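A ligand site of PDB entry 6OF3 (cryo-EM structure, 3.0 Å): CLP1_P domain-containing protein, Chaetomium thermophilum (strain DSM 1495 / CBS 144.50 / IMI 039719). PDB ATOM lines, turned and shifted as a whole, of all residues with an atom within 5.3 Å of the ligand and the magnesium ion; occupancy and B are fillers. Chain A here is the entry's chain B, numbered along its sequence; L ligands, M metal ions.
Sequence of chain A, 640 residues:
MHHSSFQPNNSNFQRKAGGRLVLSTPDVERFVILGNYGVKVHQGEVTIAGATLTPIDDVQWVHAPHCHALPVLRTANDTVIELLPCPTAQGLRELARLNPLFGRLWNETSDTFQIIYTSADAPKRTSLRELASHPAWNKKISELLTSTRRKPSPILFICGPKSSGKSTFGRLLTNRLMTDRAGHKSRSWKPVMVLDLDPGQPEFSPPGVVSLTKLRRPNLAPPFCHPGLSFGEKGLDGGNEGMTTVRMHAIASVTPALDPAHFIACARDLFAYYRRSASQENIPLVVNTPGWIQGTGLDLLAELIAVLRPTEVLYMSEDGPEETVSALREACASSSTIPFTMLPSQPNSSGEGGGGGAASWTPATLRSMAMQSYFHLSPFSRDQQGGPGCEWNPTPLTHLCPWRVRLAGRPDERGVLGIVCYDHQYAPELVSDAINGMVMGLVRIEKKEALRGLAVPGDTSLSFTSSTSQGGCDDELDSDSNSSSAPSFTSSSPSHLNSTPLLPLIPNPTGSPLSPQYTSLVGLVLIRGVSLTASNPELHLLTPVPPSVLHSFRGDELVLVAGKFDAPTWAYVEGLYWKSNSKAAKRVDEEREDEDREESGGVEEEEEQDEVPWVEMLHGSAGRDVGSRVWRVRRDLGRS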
ATOM      1  N   HIS A  68     -18.931  14.012  13.589  1.00  0.00           N
ATOM      2  CA  HIS A  68     -19.292  14.004  12.181  1.00  0.00           C
ATOM      3  C   HIS A  68     -19.242  15.395  11.553  1.00  0.00           C
ATOM      4  O   HIS A  68     -18.675  16.331  12.130  1.00  0.00           O
ATOM      5  CB  HIS A  68     -20.682  13.402  11.966  1.00  0.00           C
ATOM      6  CG  HIS A  68     -20.812  11.964  12.378  1.00  0.00           C
ATOM      7  ND1 HIS A  68     -20.448  11.505  13.621  1.00  0.00           N
ATOM      8  CD2 HIS A  68     -21.284  10.898  11.694  1.00  0.00           C
ATOM      9  CE1 HIS A  68     -20.684  10.207  13.690  1.00  0.00           C
ATOM     10  NE2 HIS A  68     -21.185   9.810  12.538  1.00  0.00           N
ATOM     11  N   ALA A  69     -19.864  15.535  10.388  1.00  0.00           N
ATOM     12  CA  ALA A  69     -19.894  16.807   9.676  1.00  0.00           C
ATOM     13  C   ALA A  69     -20.977  17.696  10.268  1.00  0.00           C
ATOM     14  O   ALA A  69     -22.171  17.415  10.100  1.00  0.00           O
ATOM     15  CB  ALA A  69     -20.122  16.572   8.190  1.00  0.00           C
ATOM     16  N   ARG A 129     -14.485  19.388  11.007  1.00  0.00           N
ATOM     17  CA  ARG A 129     -14.930  19.271   9.624  1.00  0.00           C
ATOM     18  C   ARG A 129     -16.155  20.156   9.377  1.00  0.00           C
ATOM     19  O   ARG A 129     -16.588  20.941  10.223  1.00  0.00           O
ATOM     20  CB  ARG A 129     -15.243  17.816   9.300  1.00  0.00           C
ATOM     21  CG  ARG A 129     -14.156  16.870   9.752  1.00  0.00           C
ATOM     22  CD  ARG A 129     -14.609  15.414   9.640  1.00  0.00           C
ATOM     23  NE  ARG A 129     -13.655  14.522  10.271  1.00  0.00           N
ATOM     24  CZ  ARG A 129     -13.803  13.198  10.341  1.00  0.00           C
ATOM     25  NH1 ARG A 129     -14.874  12.621   9.829  1.00  0.00           N
ATOM     26  NH2 ARG A 129     -12.886  12.453  10.938  1.00  0.00           N
ATOM     27  N   GLU A 130     -16.802  19.941   8.226  1.00  0.00           N
ATOM     28  CA  GLU A 130     -17.979  20.723   7.869  1.00  0.00           C
ATOM     29  C   GLU A 130     -18.716  20.049   6.720  1.00  0.00           C
ATOM     30  O   GLU A 130     -18.074  19.625   5.754  1.00  0.00           O
ATOM     31  CB  GLU A 130     -17.581  22.152   7.461  1.00  0.00           C
ATOM     32  CG  GLU A 130     -18.713  23.005   6.993  1.00  0.00           C
ATOM     33  CD  GLU A 130     -18.247  24.369   6.549  1.00  0.00           C
ATOM     34  OE1 GLU A 130     -17.754  25.131   7.398  1.00  0.00           O
ATOM     35  OE2 GLU A 130     -18.395  24.692   5.355  1.00  0.00           O
ATOM     36  N   LEU A 131     -20.031  19.951   6.831  1.00  0.00           N
ATOM     37  CA  LEU A 131     -20.842  19.333   5.798  1.00  0.00           C
ATOM     38  C   LEU A 131     -20.910  20.254   4.580  1.00  0.00           C
ATOM     39  O   LEU A 131     -21.349  21.404   4.693  1.00  0.00           O
ATOM     40  CB  LEU A 131     -22.248  19.043   6.319  1.00  0.00           C
ATOM     41  CG  LEU A 131     -23.212  18.456   5.276  1.00  0.00           C
ATOM     42  CD1 LEU A 131     -22.676  17.134   4.761  1.00  0.00           C
ATOM     43  CD2 LEU A 131     -24.592  18.284   5.855  1.00  0.00           C
ATOM     44  N   ALA A 132     -20.482  19.740   3.434  1.00  0.00           N
ATOM     45  CA  ALA A 132     -20.509  20.497   2.191  1.00  0.00           C
ATOM     46  C   ALA A 132     -21.121  19.620   1.110  1.00  0.00           C
ATOM     47  O   ALA A 132     -20.673  18.487   0.912  1.00  0.00           O
ATOM     48  CB  ALA A 132     -19.114  20.965   1.781  1.00  0.00           C
ATOM     49  N   SER A 133     -22.124  20.142   0.427  1.00  0.00           N
ATOM     50  CA  SER A 133     -22.828  19.391  -0.609  1.00  0.00           C
ATOM     51  C   SER A 133     -22.210  19.658  -1.968  1.00  0.00           C
ATOM     52  O   SER A 133     -22.160  20.809  -2.413  1.00  0.00           O
ATOM     53  CB  SER A 133     -24.313  19.757  -0.618  1.00  0.00           C
ATOM     54  OG  SER A 133     -24.479  21.112  -0.974  1.00  0.00           O
ATOM     55  N   HIS A 134     -21.733  18.595  -2.610  1.00  0.00           N
ATOM     56  CA  HIS A 134     -21.184  18.689  -3.945  1.00  0.00           C
ATOM     57  C   HIS A 134     -22.299  19.070  -4.930  1.00  0.00           C
ATOM     58  O   HIS A 134     -23.476  18.753  -4.681  1.00  0.00           O
ATOM     59  CB  HIS A 134     -20.580  17.344  -4.337  1.00  0.00           C
ATOM     60  CG  HIS A 134     -19.434  16.937  -3.462  1.00  0.00           C
ATOM     61  ND1 HIS A 134     -18.235  17.621  -3.432  1.00  0.00           N
ATOM     62  CD2 HIS A 134     -19.305  15.923  -2.562  1.00  0.00           C
ATOM     63  CE1 HIS A 134     -17.424  17.037  -2.572  1.00  0.00           C
ATOM     64  NE2 HIS A 134     -18.045  16.008  -2.032  1.00  0.00           N
ATOM     65  N   TRP A 137     -24.313  15.824  -6.389  1.00  0.00           N
ATOM     66  CA  TRP A 137     -25.214  15.279  -5.366  1.00  0.00           C
ATOM     67  C   TRP A 137     -26.532  16.045  -5.296  1.00  0.00           C
ATOM     68  O   TRP A 137     -27.615  15.457  -5.381  1.00  0.00           O
ATOM     69  CB  TRP A 137     -24.534  15.346  -4.007  1.00  0.00           C
ATOM     70  CG  TRP A 137     -23.561  14.260  -3.721  1.00  0.00           C
ATOM     71  CD1 TRP A 137     -22.899  13.514  -4.627  1.00  0.00           C
ATOM     72  CD2 TRP A 137     -23.106  13.842  -2.438  1.00  0.00           C
ATOM     73  NE1 TRP A 137     -22.069  12.618  -3.990  1.00  0.00           N
ATOM     74  CE2 TRP A 137     -22.177  12.809  -2.643  1.00  0.00           C
ATOM     75  CE3 TRP A 137     -23.399  14.236  -1.134  1.00  0.00           C
ATOM     76  CZ2 TRP A 137     -21.539  12.163  -1.592  1.00  0.00           C
ATOM     77  CZ3 TRP A 137     -22.766  13.587  -0.091  1.00  0.00           C
ATOM     78  CH2 TRP A 137     -21.851  12.568  -0.328  1.00  0.00           C
ATOM     79  N   PRO A 161     -18.932   1.138  -2.159  1.00  0.00           N
ATOM     80  CA  PRO A 161     -17.790   0.750  -1.338  1.00  0.00           C
ATOM     81  C   PRO A 161     -17.706   1.538  -0.038  1.00  0.00           C
ATOM     82  O   PRO A 161     -18.258   2.640   0.064  1.00  0.00           O
ATOM     83  CB  PRO A 161     -16.594   1.040  -2.239  1.00  0.00           C
ATOM     84  CG  PRO A 161     -17.067   2.208  -3.016  1.00  0.00           C
ATOM     85  CD  PRO A 161     -18.465   1.796  -3.394  1.00  0.00           C
ATOM     86  N   LYS A 162     -17.063   0.930   0.974  1.00  0.00           N
ATOM     87  CA  LYS A 162     -16.856   1.494   2.311  1.00  0.00           C
ATOM     88  C   LYS A 162     -16.369   2.940   2.282  1.00  0.00           C
ATOM     89  O   LYS A 162     -15.626   3.301   1.366  1.00  0.00           O
ATOM     90  CB  LYS A 162     -15.857   0.652   3.094  1.00  0.00           C
ATOM     91  CG  LYS A 162     -16.350  -0.715   3.471  1.00  0.00           C
ATOM     92  CD  LYS A 162     -15.337  -1.412   4.359  1.00  0.00           C
ATOM     93  CE  LYS A 162     -15.810  -2.790   4.776  1.00  0.00           C
ATOM     94  NZ  LYS A 162     -14.795  -3.494   5.617  1.00  0.00           N
ATOM     95  N   SER A 163     -16.680   3.687   3.355  1.00  0.00           N
ATOM     96  CA  SER A 163     -16.386   5.099   3.582  1.00  0.00           C
ATOM     97  C   SER A 163     -16.435   5.936   2.316  1.00  0.00           C
ATOM     98  O   SER A 163     -15.426   6.503   1.891  1.00  0.00           O
ATOM     99  CB  SER A 163     -15.000   5.247   4.232  1.00  0.00           C
ATOM    100  OG  SER A 163     -14.978   4.617   5.500  1.00  0.00           O
ATOM    101  N   SER A 164     -17.617   6.022   1.710  1.00  0.00           N
ATOM    102  CA  SER A 164     -17.815   6.777   0.491  1.00  0.00           C
ATOM    103  C   SER A 164     -18.856   7.869   0.627  1.00  0.00           C
ATOM    104  O   SER A 164     -18.823   8.828  -0.153  1.00  0.00           O
ATOM    105  CB  SER A 164     -18.216   5.859  -0.664  1.00  0.00           C
ATOM    106  OG  SER A 164     -19.434   5.209  -0.385  1.00  0.00           O
ATOM    107  N   GLY A 165     -19.789   7.758   1.563  1.00  0.00           N
ATOM    108  CA  GLY A 165     -20.801   8.768   1.742  1.00  0.00           C
ATOM    109  C   GLY A 165     -22.222   8.275   1.563  1.00  0.00           C
ATOM    110  O   GLY A 165     -23.114   9.071   1.277  1.00  0.00           O
ATOM    111  N   LYS A 166     -22.400   6.956   1.651  1.00  0.00           N
ATOM    112  CA  LYS A 166     -23.732   6.346   1.536  1.00  0.00           C
ATOM    113  C   LYS A 166     -24.699   6.904   2.571  1.00  0.00           C
ATOM    114  O   LYS A 166     -25.817   7.328   2.238  1.00  0.00           O
ATOM    115  CB  LYS A 166     -23.635   4.840   1.689  1.00  0.00           C
ATOM    116  CG  LYS A 166     -22.903   4.113   0.597  1.00  0.00           C
ATOM    117  CD  LYS A 166     -22.691   2.680   0.997  1.00  0.00           C
ATOM    118  CE  LYS A 166     -21.880   2.615   2.276  1.00  0.00           C
ATOM    119  NZ  LYS A 166     -21.553   1.245   2.692  1.00  0.00           N
ATOM    120  N   SER A 167     -24.285   6.871   3.849  1.00  0.00           N
ATOM    121  CA  SER A 167     -25.104   7.341   4.964  1.00  0.00           C
ATOM    122  C   SER A 167     -25.482   8.810   4.806  1.00  0.00           C
ATOM    123  O   SER A 167     -26.649   9.168   4.965  1.00  0.00           O
ATOM    124  CB  SER A 167     -24.358   7.107   6.274  1.00  0.00           C
ATOM    125  OG  SER A 167     -24.248   5.719   6.554  1.00  0.00           O
ATOM    126  N   THR A 168     -24.471   9.674   4.620  1.00  0.00           N
ATOM    127  CA  THR A 168     -24.665  11.111   4.439  1.00  0.00           C
ATOM    128  C   THR A 168     -25.679  11.420   3.339  1.00  0.00           C
ATOM    129  O   THR A 168     -26.576  12.254   3.498  1.00  0.00           O
ATOM    130  CB  THR A 168     -23.332  11.781   4.131  1.00  0.00           C
ATOM    131  OG1 THR A 168     -22.444  11.563   5.235  1.00  0.00           O
ATOM    132  CG2 THR A 168     -23.506  13.269   3.923  1.00  0.00           C
ATOM    133  N   PHE A 169     -25.482  10.803   2.176  1.00  0.00           N
ATOM    134  CA  PHE A 169     -26.390  10.976   1.049  1.00  0.00           C
ATOM    135  C   PHE A 169     -27.808  10.563   1.420  1.00  0.00           C
ATOM    136  O   PHE A 169     -28.778  11.231   1.039  1.00  0.00           O
ATOM    137  CB  PHE A 169     -25.902  10.187  -0.149  1.00  0.00           C
ATOM    138  CG  PHE A 169     -26.704  10.427  -1.364  1.00  0.00           C
ATOM    139  CD1 PHE A 169     -26.914  11.716  -1.795  1.00  0.00           C
ATOM    140  CD2 PHE A 169     -27.218   9.395  -2.093  1.00  0.00           C
ATOM    141  CE1 PHE A 169     -27.639  11.972  -2.917  1.00  0.00           C
ATOM    142  CE2 PHE A 169     -27.946   9.636  -3.221  1.00  0.00           C
ATOM    143  CZ  PHE A 169     -28.162  10.926  -3.636  1.00  0.00           C
ATOM    144  N   ASP A 198     -28.105  -2.705   7.705  1.00  0.00           N
ATOM    145  CA  ASP A 198     -26.693  -2.628   8.041  1.00  0.00           C
ATOM    146  C   ASP A 198     -26.470  -3.053   9.487  1.00  0.00           C
ATOM    147  O   ASP A 198     -26.616  -2.233  10.396  1.00  0.00           O
ATOM    148  CB  ASP A 198     -26.194  -1.191   7.811  1.00  0.00           C
ATOM    149  CG  ASP A 198     -24.677  -1.011   8.012  1.00  0.00           C
ATOM    150  OD1 ASP A 198     -24.124  -1.265   9.109  1.00  0.00           O
ATOM    151  OD2 ASP A 198     -24.031  -0.553   7.055  1.00  0.00           O
ATOM    152  N   GLN A 201     -22.998  -1.020  11.390  1.00  0.00           N
ATOM    153  CA  GLN A 201     -23.143   0.316  11.969  1.00  0.00           C
ATOM    154  C   GLN A 201     -24.534   0.777  11.590  1.00  0.00           C
ATOM    155  O   GLN A 201     -24.729   1.498  10.600  1.00  0.00           O
ATOM    156  CB  GLN A 201     -22.055   1.261  11.476  1.00  0.00           C
ATOM    157  CG  GLN A 201     -22.068   2.611  12.151  1.00  0.00           C
ATOM    158  CD  GLN A 201     -20.963   3.500  11.651  1.00  0.00           C
ATOM    159  OE1 GLN A 201     -19.777   3.146  11.712  1.00  0.00           O
ATOM    160  NE2 GLN A 201     -21.322   4.669  11.131  1.00  0.00           N
ATOM    161  N   PRO A 290     -25.158  -2.600   3.744  1.00  0.00           N
ATOM    162  CA  PRO A 290     -23.876  -2.557   4.467  1.00  0.00           C
ATOM    163  C   PRO A 290     -22.712  -1.940   3.719  1.00  0.00           C
ATOM    164  O   PRO A 290     -22.072  -1.004   4.201  1.00  0.00           O
ATOM    165  CB  PRO A 290     -23.609  -4.041   4.762  1.00  0.00           C
ATOM    166  CG  PRO A 290     -24.935  -4.568   4.949  1.00  0.00           C
ATOM    167  CD  PRO A 290     -25.709  -3.970   3.828  1.00  0.00           C
ATOM    168  N   GLN A 346     -15.989  11.361  -1.720  1.00  0.00           N
ATOM    169  CA  GLN A 346     -14.980  12.247  -1.128  1.00  0.00           C
ATOM    170  C   GLN A 346     -14.248  11.546   0.003  1.00  0.00           C
ATOM    171  O   GLN A 346     -14.857  10.819   0.798  1.00  0.00           O
ATOM    172  CB  GLN A 346     -15.598  13.536  -0.575  1.00  0.00           C
ATOM    173  CG  GLN A 346     -14.606  14.598  -0.173  1.00  0.00           C
ATOM    174  CD  GLN A 346     -15.163  15.994  -0.316  1.00  0.00           C
ATOM    175  OE1 GLN A 346     -16.150  16.349   0.328  1.00  0.00           O
ATOM    176  NE2 GLN A 346     -14.540  16.795  -1.168  1.00  0.00           N
HETATM  177  P1  LIG L   1     -19.886   3.587   6.292  1.00  0.00           P
HETATM  178  S1  LIG L   1     -20.341   3.554   8.173  1.00  0.00           S
HETATM  179  O1  LIG L   1     -18.757   2.645   5.980  1.00  0.00           O
HETATM  180  O2  LIG L   1     -21.092   3.250   5.462  1.00  0.00           O
HETATM  181  P2  LIG L   1     -20.336   5.642   4.543  1.00  0.00           P
HETATM  182  O3  LIG L   1     -19.721   5.030   3.320  1.00  0.00           O
HETATM  183  O4  LIG L   1     -21.809   5.465   4.779  1.00  0.00           O
HETATM  184  O5  LIG L   1     -19.536   5.074   5.810  1.00  0.00           O
HETATM  185  P3  LIG L   1     -20.752   8.145   5.565  1.00  0.00           P
HETATM  186  O6  LIG L   1     -21.911   8.789   4.846  1.00  0.00           O
HETATM  187  O7  LIG L   1     -21.009   7.333   6.798  1.00  0.00           O
HETATM  188  O8  LIG L   1     -19.980   7.202   4.526  1.00  0.00           O
HETATM  189  O9  LIG L   1     -19.695   9.293   5.911  1.00  0.00           O
HETATM  190  C1  LIG L   1     -18.311   9.029   6.039  1.00  0.00           C
HETATM  191  C2  LIG L   1     -17.663  10.355   6.310  1.00  0.00           C
HETATM  192  O10 LIG L   1     -17.535  11.106   5.093  1.00  0.00           O
HETATM  193  C3  LIG L   1     -18.444  11.240   7.275  1.00  0.00           C
HETATM  194  O11 LIG L   1     -17.757  11.395   8.491  1.00  0.00           O
HETATM  195  C4  LIG L   1     -18.675  12.545   6.534  1.00  0.00           C
HETATM  196  O12 LIG L   1     -18.294  13.637   7.354  1.00  0.00           O
HETATM  197  C5  LIG L   1     -17.681  12.472   5.382  1.00  0.00           C
HETATM  198  N1  LIG L   1     -18.087  13.181   4.151  1.00  0.00           N
HETATM  199  C6  LIG L   1     -18.152  12.633   2.901  1.00  0.00           C
HETATM  200  N2  LIG L   1     -18.541  13.454   1.968  1.00  0.00           N
HETATM  201  C7  LIG L   1     -18.745  14.641   2.655  1.00  0.00           C
HETATM  202  C8  LIG L   1     -19.170  15.915   2.231  1.00  0.00           C
HETATM  203  N3  LIG L   1     -19.480  16.207   0.968  1.00  0.00           N
HETATM  204  N4  LIG L   1     -19.278  16.885   3.156  1.00  0.00           N
HETATM  205  C9  LIG L   1     -18.975  16.600   4.422  1.00  0.00           C
HETATM  206  N5  LIG L   1     -18.573  15.453   4.932  1.00  0.00           N
HETATM  207  C10 LIG L   1     -18.477  14.487   4.001  1.00  0.00           C
HETATM  208 MG    MG M   1     -22.406   4.543   6.520  1.00  0.00          MG
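The magnesium ion is bound by an oxygen (O4) of the ligand (2.1 Å), an oxygen (O2) of the ligand (2.1 Å) and the side-chain hydroxyl of Ser 167 (2.2 Å). The magnesium ion has three donor atoms within binding distance. Slightly farther from the magnesium ion lies S1 of the ligand (2.8 Å).
CB of Ala 69 touches O12 of the ligand (3.6 Å). Glu 130 touches the ligand (O to C9, 3.4 Å). Leu 131 touches the ligand. Hydrophobic or aromatic side chains that line the ligand: Ala 69, Leu 131 and His 134. Of the 22 residues printed, 14 come within 4 Å of the ligand. The nearest printed residue that does not touch the ligand is Lys 162 (4.1 Å).
The side-chain hydroxyl (OG) of Ser 164 sits at hydrogen-bond distance from the backbone carbonyl oxygen (O) of Pro 161 (2.9 Å). The side-chain amino group of Lys 166 sits at hydrogen-bond distance from the backbone carbonyl oxygen of Pro 290 (2.8 Å). The side-chain amide oxygen (OE1) of Gln 346 is in hydrogen-bond range of a ring nitrogen (NE2) of His 134, 3.0 Å away. N of Gln 201 is in hydrogen-bond range of OD1 of Asp 198 (2.6 Å).
Within 4 Å of the magnesium ion: Ser 167.
The backbone NH of Ser 167 lies within hydrogen-bond range of an oxygen (O6) of the ligand, 3.2 Å away. An oxygen (O8) of the ligand sits at hydrogen-bond distance from the backbone NH (N) of Gly 165 (3.0 Å). OE1 of Gln 346 lies within hydrogen-bond range of N3 of the ligand (3.4 Å). S1 of the ligand lies close to NE2 of Gln 201 (3.3 Å). An oxygen (O6) of the ligand sits at hydrogen-bond distance from the backbone NH (N) of Thr 168 (2.7 Å). The backbone NH (N) of Ser 164 lies within hydrogen-bond range of an oxygen (O3) of the ligand, at 2.8 Å. The backbone carbonyl oxygen of Ala 132 is in hydrogen-bond range of a nitrogen (N3) of the ligand, 2.6 Å away. NH1 of Arg 129 sits at hydrogen-bond distance from O11 of the ligand (3.4 Å). A nitrogen (N4) of the ligand sits at hydrogen-bond distance from the backbone NH (N) of Ala 132 (3.1 Å). A ring nitrogen (NE2) of His 134 sits at hydrogen-bond distance from a nitrogen (N3) of the ligand (3.3 Å). The side-chain hydroxyl (OG1) of Thr 168 lies within hydrogen-bond range of an oxygen (O6) of the ligand. NZ of Lys 166 lies close to O2 of the ligand. The backbone NH (N) of Ser 163 sits at hydrogen-bond distance from an oxygen (O3) of the ligand, at 3.3 Å.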
